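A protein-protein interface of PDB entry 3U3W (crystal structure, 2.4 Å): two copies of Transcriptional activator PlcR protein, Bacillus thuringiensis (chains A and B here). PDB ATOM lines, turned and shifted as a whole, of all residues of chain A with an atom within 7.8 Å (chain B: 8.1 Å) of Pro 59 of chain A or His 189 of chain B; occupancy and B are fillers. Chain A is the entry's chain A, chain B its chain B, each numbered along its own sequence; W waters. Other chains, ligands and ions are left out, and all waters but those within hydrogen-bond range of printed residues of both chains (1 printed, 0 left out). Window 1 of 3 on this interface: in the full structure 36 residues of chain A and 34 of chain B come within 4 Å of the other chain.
Water W1 lies within hydrogen-bond range of the backbone carbonyl oxygen (O) of Gln 57 of chain A (2.7 Å) and the backbone NH (N) of His 189 of chain B (3.0 Å).
Ile 60 of chain A touches Ile 61 of chain B, and with the chains exchanged Ile 61 of chain A touches Ile 60 of chain B.
A ring nitrogen (NE2) of His 62 of chain A lies within hydrogen-bond range of the side-chain carboxylate of Glu 9 of chain A (2.7 Å). The backbone carbonyl oxygen of Leu 56 of chain A lies within hydrogen-bond range of the guanidinium group of Arg 17 of chain A, 3.1 Å away. N of Ile 58 of chain A sits at hydrogen-bond distance from O of Ala 53 of chain A (2.9 Å). OH of Tyr 152 of chain B sits at hydrogen-bond distance from O of His 189 of chain B (2.5 Å).
Of the 17 printed residues of chain A, 8 touch a printed residue of chain B. Printed residues of chain A that touch a printed residue of chain B: Arg 17, Gln 57, Ile 58, Pro 59, Ile 60, Ile 61, His 62 and Tyr 64. Along chain B the printed residues that touch a printed residue of chain A span positions 60 to 189. Among the printed residues, no Asp or Glu carboxylate lies within 4 Å of a Lys or Arg side-chain nitrogen of the other chain.
Of the printed residues of chain B, Arg 17 of chain A touches Ala 187 and Leu 188. Pro 59 of chain A touches just one residue of chain B: His 189 (3.9 Å). Of the printed residues of chain B, His 62 of chain A touches His 189. Ile 149 of chain B touches none of the printed residues of chain A. Printed residues of chain A within 4 Å of Val 151 of chain B: Gln 57 and Ile 58. Of chain A, only Pro 59 and His 62 come within 4 Å of His 189 of chain B. Asp 190 of chain B touches none of the printed residues of chain A. The nearest printed residue of chain A that does not touch Ile 60 of chain B is Ile 60 of chain A (5.4 Å).
Among the printed residues, merely in contact across the chains: Tyr 64 of chain A with Ile 60 of chain B (3.2 Å), Gln 57 of chain A with Val 151 of chain B (3.6 Å), Gln 57 of chain A with Leu 188 of chain B (3.7 Å), Ile 61 of chain A with Ile 60 of chain B (3.7 Å), Arg 17 of chain A with Leu 188 of chain B (3.8 Å), Ile 60 of chain A with Ile 61 of chain B (3.8 Å), Ile 58 of chain A with Val 151 of chain B (3.8 Å), Pro 59 of chain A with His 189 of chain B (3.9 Å), His 62 of chain A with His 189 of chain B (3.9 Å) and Arg 17 of chain A with Ala 187 of chain B (3.9 Å).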
ATOM      1  N   GLU A   9      -9.503   6.750  13.527  1.00  0.00           N
ATOM      2  CA  GLU A   9      -9.785   5.333  13.693  1.00  0.00           C
ATOM      3  C   GLU A   9      -8.478   4.563  13.924  1.00  0.00           C
ATOM      4  O   GLU A   9      -8.393   3.672  14.777  1.00  0.00           O
ATOM      5  CB  GLU A   9     -10.534   4.795  12.473  1.00  0.00           C
ATOM      6  CG  GLU A   9     -11.031   3.364  12.628  1.00  0.00           C
ATOM      7  CD  GLU A   9     -12.092   3.220  13.712  1.00  0.00           C
ATOM      8  OE1 GLU A   9     -12.573   4.257  14.225  1.00  0.00           O
ATOM      9  OE2 GLU A   9     -12.445   2.068  14.049  1.00  0.00           O
ATOM     10  N   ILE A  13      -7.538   2.950  17.651  1.00  0.00           N
ATOM     11  CA  ILE A  13      -7.211   1.534  17.788  1.00  0.00           C
ATOM     12  C   ILE A  13      -5.770   1.309  18.265  1.00  0.00           C
ATOM     13  O   ILE A  13      -5.487   0.333  18.962  1.00  0.00           O
ATOM     14  CB  ILE A  13      -7.476   0.756  16.468  1.00  0.00           C
ATOM     15  CG1 ILE A  13      -8.917   0.958  16.012  1.00  0.00           C
ATOM     16  CG2 ILE A  13      -7.191  -0.723  16.648  1.00  0.00           C
ATOM     17  CD1 ILE A  13      -9.214   0.379  14.660  1.00  0.00           C
ATOM     18  N   ARG A  17      -4.672  -0.388  21.814  1.00  0.00           N
ATOM     19  CA  ARG A  17      -3.741  -1.509  21.823  1.00  0.00           C
ATOM     20  C   ARG A  17      -2.500  -1.200  22.642  1.00  0.00           C
ATOM     21  O   ARG A  17      -1.622  -2.051  22.787  1.00  0.00           O
ATOM     22  CB  ARG A  17      -3.329  -1.884  20.399  1.00  0.00           C
ATOM     23  CG  ARG A  17      -4.459  -2.420  19.540  1.00  0.00           C
ATOM     24  CD  ARG A  17      -4.742  -3.903  19.786  1.00  0.00           C
ATOM     25  NE  ARG A  17      -5.685  -4.418  18.795  1.00  0.00           N
ATOM     26  CZ  ARG A  17      -7.007  -4.428  18.952  1.00  0.00           C
ATOM     27  NH1 ARG A  17      -7.550  -3.964  20.075  1.00  0.00           N
ATOM     28  NH2 ARG A  17      -7.786  -4.907  17.988  1.00  0.00           N
ATOM     29  N   ALA A  53      -2.681  -2.449   9.523  1.00  0.00           N
ATOM     30  CA  ALA A  53      -3.825  -3.322   9.767  1.00  0.00           C
ATOM     31  C   ALA A  53      -3.403  -4.641  10.402  1.00  0.00           C
ATOM     32  O   ALA A  53      -4.061  -5.148  11.306  1.00  0.00           O
ATOM     33  CB  ALA A  53      -4.605  -3.570   8.479  1.00  0.00           C
ATOM     34  N   ALA A  54      -2.298  -5.191   9.926  1.00  0.00           N
ATOM     35  CA  ALA A  54      -1.780  -6.430  10.479  1.00  0.00           C
ATOM     36  C   ALA A  54      -1.370  -6.283  11.951  1.00  0.00           C
ATOM     37  O   ALA A  54      -1.824  -7.041  12.818  1.00  0.00           O
ATOM     38  CB  ALA A  54      -0.615  -6.932   9.638  1.00  0.00           C
ATOM     39  N   LEU A  56      -2.218  -4.090  14.092  1.00  0.00           N
ATOM     40  CA  LEU A  56      -3.353  -3.731  14.937  1.00  0.00           C
ATOM     41  C   LEU A  56      -4.424  -4.824  14.938  1.00  0.00           C
ATOM     42  O   LEU A  56      -5.401  -4.744  15.682  1.00  0.00           O
ATOM     43  CB  LEU A  56      -3.965  -2.404  14.491  1.00  0.00           C
ATOM     44  CG  LEU A  56      -3.105  -1.139  14.501  1.00  0.00           C
ATOM     45  CD1 LEU A  56      -3.853   0.011  13.845  1.00  0.00           C
ATOM     46  CD2 LEU A  56      -2.700  -0.770  15.903  1.00  0.00           C
ATOM     47  N   GLN A  57      -4.230  -5.847  14.110  1.00  0.00           N
ATOM     48  CA  GLN A  57      -5.183  -6.952  14.001  1.00  0.00           C
ATOM     49  C   GLN A  57      -6.560  -6.448  13.596  1.00  0.00           C
ATOM     50  O   GLN A  57      -7.547  -6.680  14.278  1.00  0.00           O
ATOM     51  CB  GLN A  57      -5.260  -7.757  15.304  1.00  0.00           C
ATOM     52  CG  GLN A  57      -3.928  -8.422  15.700  1.00  0.00           C
ATOM     53  CD  GLN A  57      -4.003  -9.208  17.015  1.00  0.00           C
ATOM     54  OE1 GLN A  57      -3.679  -8.685  18.085  1.00  0.00           O
ATOM     55  NE2 GLN A  57      -4.425 -10.469  16.932  1.00  0.00           N
ATOM     56  N   ILE A  58      -6.612  -5.744  12.476  1.00  0.00           N
ATOM     57  CA  ILE A  58      -7.867  -5.209  11.970  1.00  0.00           C
ATOM     58  C   ILE A  58      -8.033  -5.620  10.514  1.00  0.00           C
ATOM     59  O   ILE A  58      -7.137  -5.380   9.703  1.00  0.00           O
ATOM     60  CB  ILE A  58      -7.886  -3.675  12.066  1.00  0.00           C
ATOM     61  CG1 ILE A  58      -7.699  -3.219  13.521  1.00  0.00           C
ATOM     62  CG2 ILE A  58      -9.152  -3.112  11.412  1.00  0.00           C
ATOM     63  CD1 ILE A  58      -8.934  -3.377  14.420  1.00  0.00           C
ATOM     64  N   PRO A  59      -9.166  -6.265  10.180  1.00  0.00           N
ATOM     65  CA  PRO A  59      -9.478  -6.563   8.779  1.00  0.00           C
ATOM     66  C   PRO A  59      -9.351  -5.284   7.969  1.00  0.00           C
ATOM     67  O   PRO A  59      -9.864  -4.230   8.359  1.00  0.00           O
ATOM     68  CB  PRO A  59     -10.940  -7.017   8.827  1.00  0.00           C
ATOM     69  CG  PRO A  59     -11.120  -7.535  10.202  1.00  0.00           C
ATOM     70  CD  PRO A  59     -10.238  -6.698  11.090  1.00  0.00           C
ATOM     71  N   ILE A  60      -8.649  -5.373   6.854  1.00  0.00           N
ATOM     72  CA  ILE A  60      -8.303  -4.182   6.094  1.00  0.00           C
ATOM     73  C   ILE A  60      -9.539  -3.447   5.570  1.00  0.00           C
ATOM     74  O   ILE A  60      -9.512  -2.230   5.404  1.00  0.00           O
ATOM     75  CB  ILE A  60      -7.314  -4.515   4.957  1.00  0.00           C
ATOM     76  CG1 ILE A  60      -6.042  -5.155   5.539  1.00  0.00           C
ATOM     77  CG2 ILE A  60      -6.950  -3.273   4.183  1.00  0.00           C
ATOM     78  CD1 ILE A  60      -6.219  -6.574   6.128  1.00  0.00           C
ATOM     79  N   ILE A  61     -10.625  -4.178   5.327  1.00  0.00           N
ATOM     80  CA  ILE A  61     -11.839  -3.564   4.779  1.00  0.00           C
ATOM     81  C   ILE A  61     -12.390  -2.526   5.760  1.00  0.00           C
ATOM     82  O   ILE A  61     -13.095  -1.593   5.375  1.00  0.00           O
ATOM     83  CB  ILE A  61     -12.928  -4.634   4.402  1.00  0.00           C
ATOM     84  CG1 ILE A  61     -14.152  -3.986   3.739  1.00  0.00           C
ATOM     85  CG2 ILE A  61     -13.353  -5.459   5.619  1.00  0.00           C
ATOM     86  CD1 ILE A  61     -13.871  -3.300   2.421  1.00  0.00           C
ATOM     87  N   HIS A  62     -12.034  -2.684   7.031  1.00  0.00           N
ATOM     88  CA  HIS A  62     -12.473  -1.750   8.052  1.00  0.00           C
ATOM     89  C   HIS A  62     -12.005  -0.331   7.766  1.00  0.00           C
ATOM     90  O   HIS A  62     -12.750   0.625   7.942  1.00  0.00           O
ATOM     91  CB  HIS A  62     -11.988  -2.176   9.432  1.00  0.00           C
ATOM     92  CG  HIS A  62     -12.421  -1.251  10.525  1.00  0.00           C
ATOM     93  ND1 HIS A  62     -13.744  -0.935  10.749  1.00  0.00           N
ATOM     94  CD2 HIS A  62     -11.708  -0.557  11.442  1.00  0.00           C
ATOM     95  CE1 HIS A  62     -13.829  -0.097  11.765  1.00  0.00           C
ATOM     96  NE2 HIS A  62     -12.609   0.146  12.208  1.00  0.00           N
ATOM     97  N   PHE A  63     -10.764  -0.183   7.335  1.00  0.00           N
ATOM     98  CA  PHE A  63     -10.251   1.153   7.094  1.00  0.00           C
ATOM     99  C   PHE A  63     -10.882   1.765   5.854  1.00  0.00           C
ATOM    100  O   PHE A  63     -11.050   2.983   5.757  1.00  0.00           O
ATOM    101  CB  PHE A  63      -8.732   1.136   7.026  1.00  0.00           C
ATOM    102  CG  PHE A  63      -8.101   0.659   8.290  1.00  0.00           C
ATOM    103  CD1 PHE A  63      -8.232   1.394   9.452  1.00  0.00           C
ATOM    104  CD2 PHE A  63      -7.410  -0.534   8.330  1.00  0.00           C
ATOM    105  CE1 PHE A  63      -7.667   0.952  10.626  1.00  0.00           C
ATOM    106  CE2 PHE A  63      -6.845  -0.981   9.502  1.00  0.00           C
ATOM    107  CZ  PHE A  63      -6.972  -0.240  10.647  1.00  0.00           C
ATOM    108  N   TYR A  64     -11.265   0.920   4.912  1.00  0.00           N
ATOM    109  CA  TYR A  64     -12.000   1.420   3.770  1.00  0.00           C
ATOM    110  C   TYR A  64     -13.431   1.810   4.149  1.00  0.00           C
ATOM    111  O   TYR A  64     -13.920   2.854   3.722  1.00  0.00           O
ATOM    112  CB  TYR A  64     -11.963   0.420   2.623  1.00  0.00           C
ATOM    113  CG  TYR A  64     -10.631   0.423   1.914  1.00  0.00           C
ATOM    114  CD1 TYR A  64     -10.414   1.242   0.810  1.00  0.00           C
ATOM    115  CD2 TYR A  64      -9.582  -0.370   2.362  1.00  0.00           C
ATOM    116  CE1 TYR A  64      -9.190   1.261   0.162  1.00  0.00           C
ATOM    117  CE2 TYR A  64      -8.357  -0.359   1.717  1.00  0.00           C
ATOM    118  CZ  TYR A  64      -8.169   0.459   0.620  1.00  0.00           C
ATOM    119  OH  TYR A  64      -6.957   0.470  -0.018  1.00  0.00           O
ATOM    120  N   GLU A  65     -14.089   0.992   4.967  1.00  0.00           N
ATOM    121  CA  GLU A  65     -15.449   1.291   5.400  1.00  0.00           C
ATOM    122  C   GLU A  65     -15.563   2.684   6.013  1.00  0.00           C
ATOM    123  O   GLU A  65     -16.428   3.475   5.625  1.00  0.00           O
ATOM    124  CB  GLU A  65     -15.947   0.242   6.395  1.00  0.00           C
ATOM    125  CG  GLU A  65     -16.301  -1.082   5.755  1.00  0.00           C
ATOM    126  CD  GLU A  65     -16.605  -2.165   6.776  1.00  0.00           C
ATOM    127  OE1 GLU A  65     -16.147  -2.039   7.936  1.00  0.00           O
ATOM    128  OE2 GLU A  65     -17.306  -3.141   6.421  1.00  0.00           O
ATOM    129  N   GLU A  73     -20.098   1.755  12.545  1.00  0.00           N
ATOM    130  CA  GLU A  73     -20.353   0.639  13.449  1.00  0.00           C
ATOM    131  C   GLU A  73     -21.847   0.501  13.696  1.00  0.00           C
ATOM    132  O   GLU A  73     -22.390  -0.597  13.646  1.00  0.00           O
ATOM    133  CB  GLU A  73     -19.601   0.805  14.775  1.00  0.00           C
ATOM    134  CG  GLU A  73     -19.959  -0.231  15.846  1.00  0.00           C
ATOM    135  CD  GLU A  73     -19.613  -1.659  15.438  1.00  0.00           C
ATOM    136  OE1 GLU A  73     -18.793  -1.839  14.508  1.00  0.00           O
ATOM    137  OE2 GLU A  73     -20.163  -2.605  16.048  1.00  0.00           O
ATOM    138  N   LYS A  76     -23.685  -0.908  10.658  1.00  0.00           N
ATOM    139  CA  LYS A  76     -23.484  -2.330  10.460  1.00  0.00           C
ATOM    140  C   LYS A  76     -24.363  -3.185  11.386  1.00  0.00           C
ATOM    141  O   LYS A  76     -24.899  -4.212  10.965  1.00  0.00           O
ATOM    142  CB  LYS A  76     -22.001  -2.683  10.581  1.00  0.00           C
ATOM    143  CG  LYS A  76     -21.142  -1.950   9.561  1.00  0.00           C
ATOM    144  CD  LYS A  76     -19.992  -2.815   9.054  1.00  0.00           C
ATOM    145  CE  LYS A  76     -19.054  -3.217  10.184  1.00  0.00           C
ATOM    146  NZ  LYS A  76     -17.967  -4.107   9.693  1.00  0.00           N
ATOM    147  N   ILE B  60     -12.155  -5.899  -1.635  1.00  0.00           N
ATOM    148  CA  ILE B  60     -10.877  -5.208  -1.727  1.00  0.00           C
ATOM    149  C   ILE B  60      -9.721  -5.986  -1.094  1.00  0.00           C
ATOM    150  O   ILE B  60      -8.563  -5.760  -1.439  1.00  0.00           O
ATOM    151  CB  ILE B  60     -10.925  -3.774  -1.165  1.00  0.00           C
ATOM    152  CG1 ILE B  60      -9.760  -2.966  -1.728  1.00  0.00           C
ATOM    153  CG2 ILE B  60     -10.859  -3.779   0.352  1.00  0.00           C
ATOM    154  CD1 ILE B  60      -9.768  -1.535  -1.302  1.00  0.00           C
ATOM    155  N   ILE B  61     -10.023  -6.897  -0.177  1.00  0.00           N
ATOM    156  CA  ILE B  61      -8.960  -7.688   0.453  1.00  0.00           C
ATOM    157  C   ILE B  61      -8.212  -8.493  -0.618  1.00  0.00           C
ATOM    158  O   ILE B  61      -7.005  -8.729  -0.515  1.00  0.00           O
ATOM    159  CB  ILE B  61      -9.499  -8.612   1.610  1.00  0.00           C
ATOM    160  CG1 ILE B  61      -8.358  -9.311   2.357  1.00  0.00           C
ATOM    161  CG2 ILE B  61     -10.473  -9.661   1.086  1.00  0.00           C
ATOM    162  CD1 ILE B  61      -7.354  -8.383   2.985  1.00  0.00           C
ATOM    163  N   GLY B 148       0.230 -10.827   9.115  1.00  0.00           N
ATOM    164  CA  GLY B 148      -0.581 -11.559   8.152  1.00  0.00           C
ATOM    165  C   GLY B 148      -2.016 -11.108   7.892  1.00  0.00           C
ATOM    166  O   GLY B 148      -2.584 -10.289   8.611  1.00  0.00           O
ATOM    167  N   ILE B 149      -2.604 -11.674   6.844  1.00  0.00           N
ATOM    168  CA  ILE B 149      -3.970 -11.369   6.444  1.00  0.00           C
ATOM    169  C   ILE B 149      -4.980 -11.973   7.415  1.00  0.00           C
ATOM    170  O   ILE B 149      -5.870 -11.266   7.893  1.00  0.00           O
ATOM    171  CB  ILE B 149      -4.276 -11.883   5.004  1.00  0.00           C
ATOM    172  CG1 ILE B 149      -3.305 -11.273   3.981  1.00  0.00           C
ATOM    173  CG2 ILE B 149      -5.730 -11.594   4.618  1.00  0.00           C
ATOM    174  CD1 ILE B 149      -3.406  -9.766   3.850  1.00  0.00           C
ATOM    175  N   VAL B 151      -6.267 -12.604  10.547  1.00  0.00           N
ATOM    176  CA  VAL B 151      -6.104 -11.966  11.832  1.00  0.00           C
ATOM    177  C   VAL B 151      -6.233 -12.957  13.015  1.00  0.00           C
ATOM    178  O   VAL B 151      -5.823 -12.648  14.116  1.00  0.00           O
ATOM    179  CB  VAL B 151      -7.127 -10.778  11.920  1.00  0.00           C
ATOM    180  CG1 VAL B 151      -7.824 -10.706  13.263  1.00  0.00           C
ATOM    181  CG2 VAL B 151      -6.452  -9.457  11.540  1.00  0.00           C
ATOM    182  N   TYR B 152      -6.770 -14.152  12.772  1.00  0.00           N
ATOM    183  CA  TYR B 152      -7.104 -15.088  13.858  1.00  0.00           C
ATOM    184  C   TYR B 152      -6.136 -16.256  14.057  1.00  0.00           C
ATOM    185  O   TYR B 152      -6.269 -17.015  15.031  1.00  0.00           O
ATOM    186  CB  TYR B 152      -8.515 -15.645  13.650  1.00  0.00           C
ATOM    187  CG  TYR B 152      -9.558 -14.560  13.652  1.00  0.00           C
ATOM    188  CD1 TYR B 152     -10.072 -14.075  14.847  1.00  0.00           C
ATOM    189  CD2 TYR B 152     -10.018 -14.004  12.462  1.00  0.00           C
ATOM    190  CE1 TYR B 152     -11.014 -13.062  14.864  1.00  0.00           C
ATOM    191  CE2 TYR B 152     -10.960 -12.986  12.470  1.00  0.00           C
ATOM    192  CZ  TYR B 152     -11.450 -12.518  13.676  1.00  0.00           C
ATOM    193  OH  TYR B 152     -12.396 -11.513  13.698  1.00  0.00           O
ATOM    194  N   LEU B 155      -4.558 -17.091  17.377  1.00  0.00           N
ATOM    195  CA  LEU B 155      -5.581 -17.598  18.295  1.00  0.00           C
ATOM    196  C   LEU B 155      -5.961 -19.054  17.989  1.00  0.00           C
ATOM    197  O   LEU B 155      -6.233 -19.843  18.889  1.00  0.00           O
ATOM    198  CB  LEU B 155      -6.816 -16.694  18.249  1.00  0.00           C
ATOM    199  CG  LEU B 155      -6.582 -15.263  18.749  1.00  0.00           C
ATOM    200  CD1 LEU B 155      -7.845 -14.417  18.602  1.00  0.00           C
ATOM    201  CD2 LEU B 155      -6.094 -15.269  20.202  1.00  0.00           C
ATOM    202  N   GLN B 184      -9.411 -12.373  24.312  1.00  0.00           N
ATOM    203  CA  GLN B 184      -8.819 -11.766  23.117  1.00  0.00           C
ATOM    204  C   GLN B 184      -9.831 -11.606  21.965  1.00  0.00           C
ATOM    205  O   GLN B 184      -9.726 -10.666  21.183  1.00  0.00           O
ATOM    206  CB  GLN B 184      -7.591 -12.553  22.647  1.00  0.00           C
ATOM    207  CG  GLN B 184      -6.425 -12.573  23.644  1.00  0.00           C
ATOM    208  CD  GLN B 184      -5.295 -13.504  23.213  1.00  0.00           C
ATOM    209  OE1 GLN B 184      -4.639 -13.263  22.197  1.00  0.00           O
ATOM    210  NE2 GLN B 184      -5.064 -14.574  23.987  1.00  0.00           N
ATOM    211  N   LEU B 185     -10.811 -12.505  21.874  1.00  0.00           N
ATOM    212  CA  LEU B 185     -11.847 -12.434  20.834  1.00  0.00           C
ATOM    213  C   LEU B 185     -12.792 -11.247  20.969  1.00  0.00           C
ATOM    214  O   LEU B 185     -13.187 -10.644  19.972  1.00  0.00           O
ATOM    215  CB  LEU B 185     -12.691 -13.705  20.821  1.00  0.00           C
ATOM    216  CG  LEU B 185     -12.084 -14.865  20.060  1.00  0.00           C
ATOM    217  CD1 LEU B 185     -13.075 -16.008  20.020  1.00  0.00           C
ATOM    218  CD2 LEU B 185     -11.720 -14.413  18.645  1.00  0.00           C
ATOM    219  N   GLU B 186     -13.185 -10.937  22.200  1.00  0.00           N
ATOM    220  CA  GLU B 186     -14.083  -9.815  22.443  1.00  0.00           C
ATOM    221  C   GLU B 186     -13.464  -8.508  21.939  1.00  0.00           C
ATOM    222  O   GLU B 186     -14.174  -7.589  21.533  1.00  0.00           O
ATOM    223  CB  GLU B 186     -14.427  -9.712  23.925  1.00  0.00           C
ATOM    224  CG  GLU B 186     -13.285  -9.245  24.795  1.00  0.00           C
ATOM    225  CD  GLU B 186     -13.673  -9.136  26.264  1.00  0.00           C
ATOM    226  OE1 GLU B 186     -14.832  -9.474  26.596  1.00  0.00           O
ATOM    227  OE2 GLU B 186     -12.818  -8.717  27.079  1.00  0.00           O
ATOM    228  N   ALA B 187     -12.136  -8.451  21.953  1.00  0.00           N
ATOM    229  CA  ALA B 187     -11.380  -7.307  21.452  1.00  0.00           C
ATOM    230  C   ALA B 187     -11.285  -7.263  19.923  1.00  0.00           C
ATOM    231  O   ALA B 187     -11.252  -6.182  19.336  1.00  0.00           O
ATOM    232  CB  ALA B 187      -9.975  -7.293  22.063  1.00  0.00           C
ATOM    233  N   LEU B 188     -11.220  -8.428  19.283  1.00  0.00           N
ATOM    234  CA  LEU B 188     -11.142  -8.485  17.830  1.00  0.00           C
ATOM    235  C   LEU B 188     -12.531  -8.476  17.191  1.00  0.00           C
ATOM    236  O   LEU B 188     -13.534  -8.767  17.832  1.00  0.00           O
ATOM    237  CB  LEU B 188     -10.375  -9.724  17.370  1.00  0.00           C
ATOM    238  CG  LEU B 188      -8.918  -9.858  17.814  1.00  0.00           C
ATOM    239  CD1 LEU B 188      -8.285 -11.084  17.168  1.00  0.00           C
ATOM    240  CD2 LEU B 188      -8.114  -8.612  17.473  1.00  0.00           C
ATOM    241  N   HIS B 189     -12.578  -8.133  15.911  1.00  0.00           N
ATOM    242  CA  HIS B 189     -13.807  -8.239  15.131  1.00  0.00           C
ATOM    243  C   HIS B 189     -14.438  -9.630  15.250  1.00  0.00           C
ATOM    244  O   HIS B 189     -13.776 -10.604  15.605  1.00  0.00           O
ATOM    245  CB  HIS B 189     -13.548  -7.868  13.663  1.00  0.00           C
ATOM    246  CG  HIS B 189     -13.452  -6.393  13.427  1.00  0.00           C
ATOM    247  ND1 HIS B 189     -13.026  -5.509  14.397  1.00  0.00           N
ATOM    248  CD2 HIS B 189     -13.730  -5.645  12.332  1.00  0.00           C
ATOM    249  CE1 HIS B 189     -13.056  -4.279  13.913  1.00  0.00           C
ATOM    250  NE2 HIS B 189     -13.476  -4.334  12.662  1.00  0.00           N
ATOM    251  N   ASP B 190     -15.721  -9.717  14.945  1.00  0.00           N
ATOM    252  CA  ASP B 190     -16.449 -10.942  15.182  1.00  0.00           C
ATOM    253  C   ASP B 190     -16.013 -12.136  14.344  1.00  0.00           C
ATOM    254  O   ASP B 190     -15.873 -12.065  13.127  1.00  0.00           O
ATOM    255  CB  ASP B 190     -17.955 -10.698  15.087  1.00  0.00           C
ATOM    256  CG  ASP B 190     -18.454  -9.754  16.187  1.00  0.00           C
ATOM    257  OD1 ASP B 190     -17.688  -9.512  17.164  1.00  0.00           O
ATOM    258  OD2 ASP B 190     -19.602  -9.256  16.061  1.00  0.00           O
ATOM    259  N   ASN B 191     -15.788 -13.236  15.050  1.00  0.00           N
ATOM    260  CA  ASN B 191     -15.513 -14.525  14.463  1.00  0.00           C
ATOM    261  C   ASN B 191     -16.277 -15.490  15.345  1.00  0.00           C
ATOM    262  O   ASN B 191     -15.703 -16.192  16.195  1.00  0.00           O
ATOM    263  CB  ASN B 191     -14.018 -14.823  14.514  1.00  0.00           C
ATOM    264  CG  ASN B 191     -13.639 -16.049  13.708  1.00  0.00           C
ATOM    265  OD1 ASN B 191     -14.505 -16.814  13.260  1.00  0.00           O
ATOM    266  ND2 ASN B 191     -12.331 -16.252  13.525  1.00  0.00           N
ATOM    267  N   GLU B 192     -17.588 -15.494  15.168  1.00  0.00           N
ATOM    268  CA  GLU B 192     -18.456 -16.208  16.087  1.00  0.00           C
ATOM    269  C   GLU B 192     -18.350 -17.737  15.963  1.00  0.00           C
ATOM    270  O   GLU B 192     -18.510 -18.453  16.950  1.00  0.00           O
ATOM    271  CB  GLU B 192     -19.883 -15.701  15.960  1.00  0.00           C
ATOM    272  CG  GLU B 192     -19.945 -14.169  15.973  1.00  0.00           C
ATOM    273  CD  GLU B 192     -21.228 -13.623  16.574  1.00  0.00           C
ATOM    274  OE1 GLU B 192     -21.525 -13.944  17.753  1.00  0.00           O
ATOM    275  OE2 GLU B 192     -21.935 -12.869  15.868  1.00  0.00           O
ATOM    276  N   ASP B 195     -15.429 -18.524  18.160  1.00  0.00           N
ATOM    277  CA  ASP B 195     -15.939 -18.354  19.506  1.00  0.00           C
ATOM    278  C   ASP B 195     -16.688 -19.606  19.964  1.00  0.00           C
ATOM    279  O   ASP B 195     -16.564 -20.027  21.108  1.00  0.00           O
ATOM    280  CB  ASP B 195     -16.877 -17.138  19.535  1.00  0.00           C
ATOM    281  CG  ASP B 195     -17.095 -16.580  20.938  1.00  0.00           C
ATOM    282  OD1 ASP B 195     -17.856 -17.182  21.737  1.00  0.00           O
ATOM    283  OD2 ASP B 195     -16.522 -15.508  21.231  1.00  0.00           O
HETATM  284  O   HOH W   1     -10.181  -7.101  14.527  1.00  0.00           O
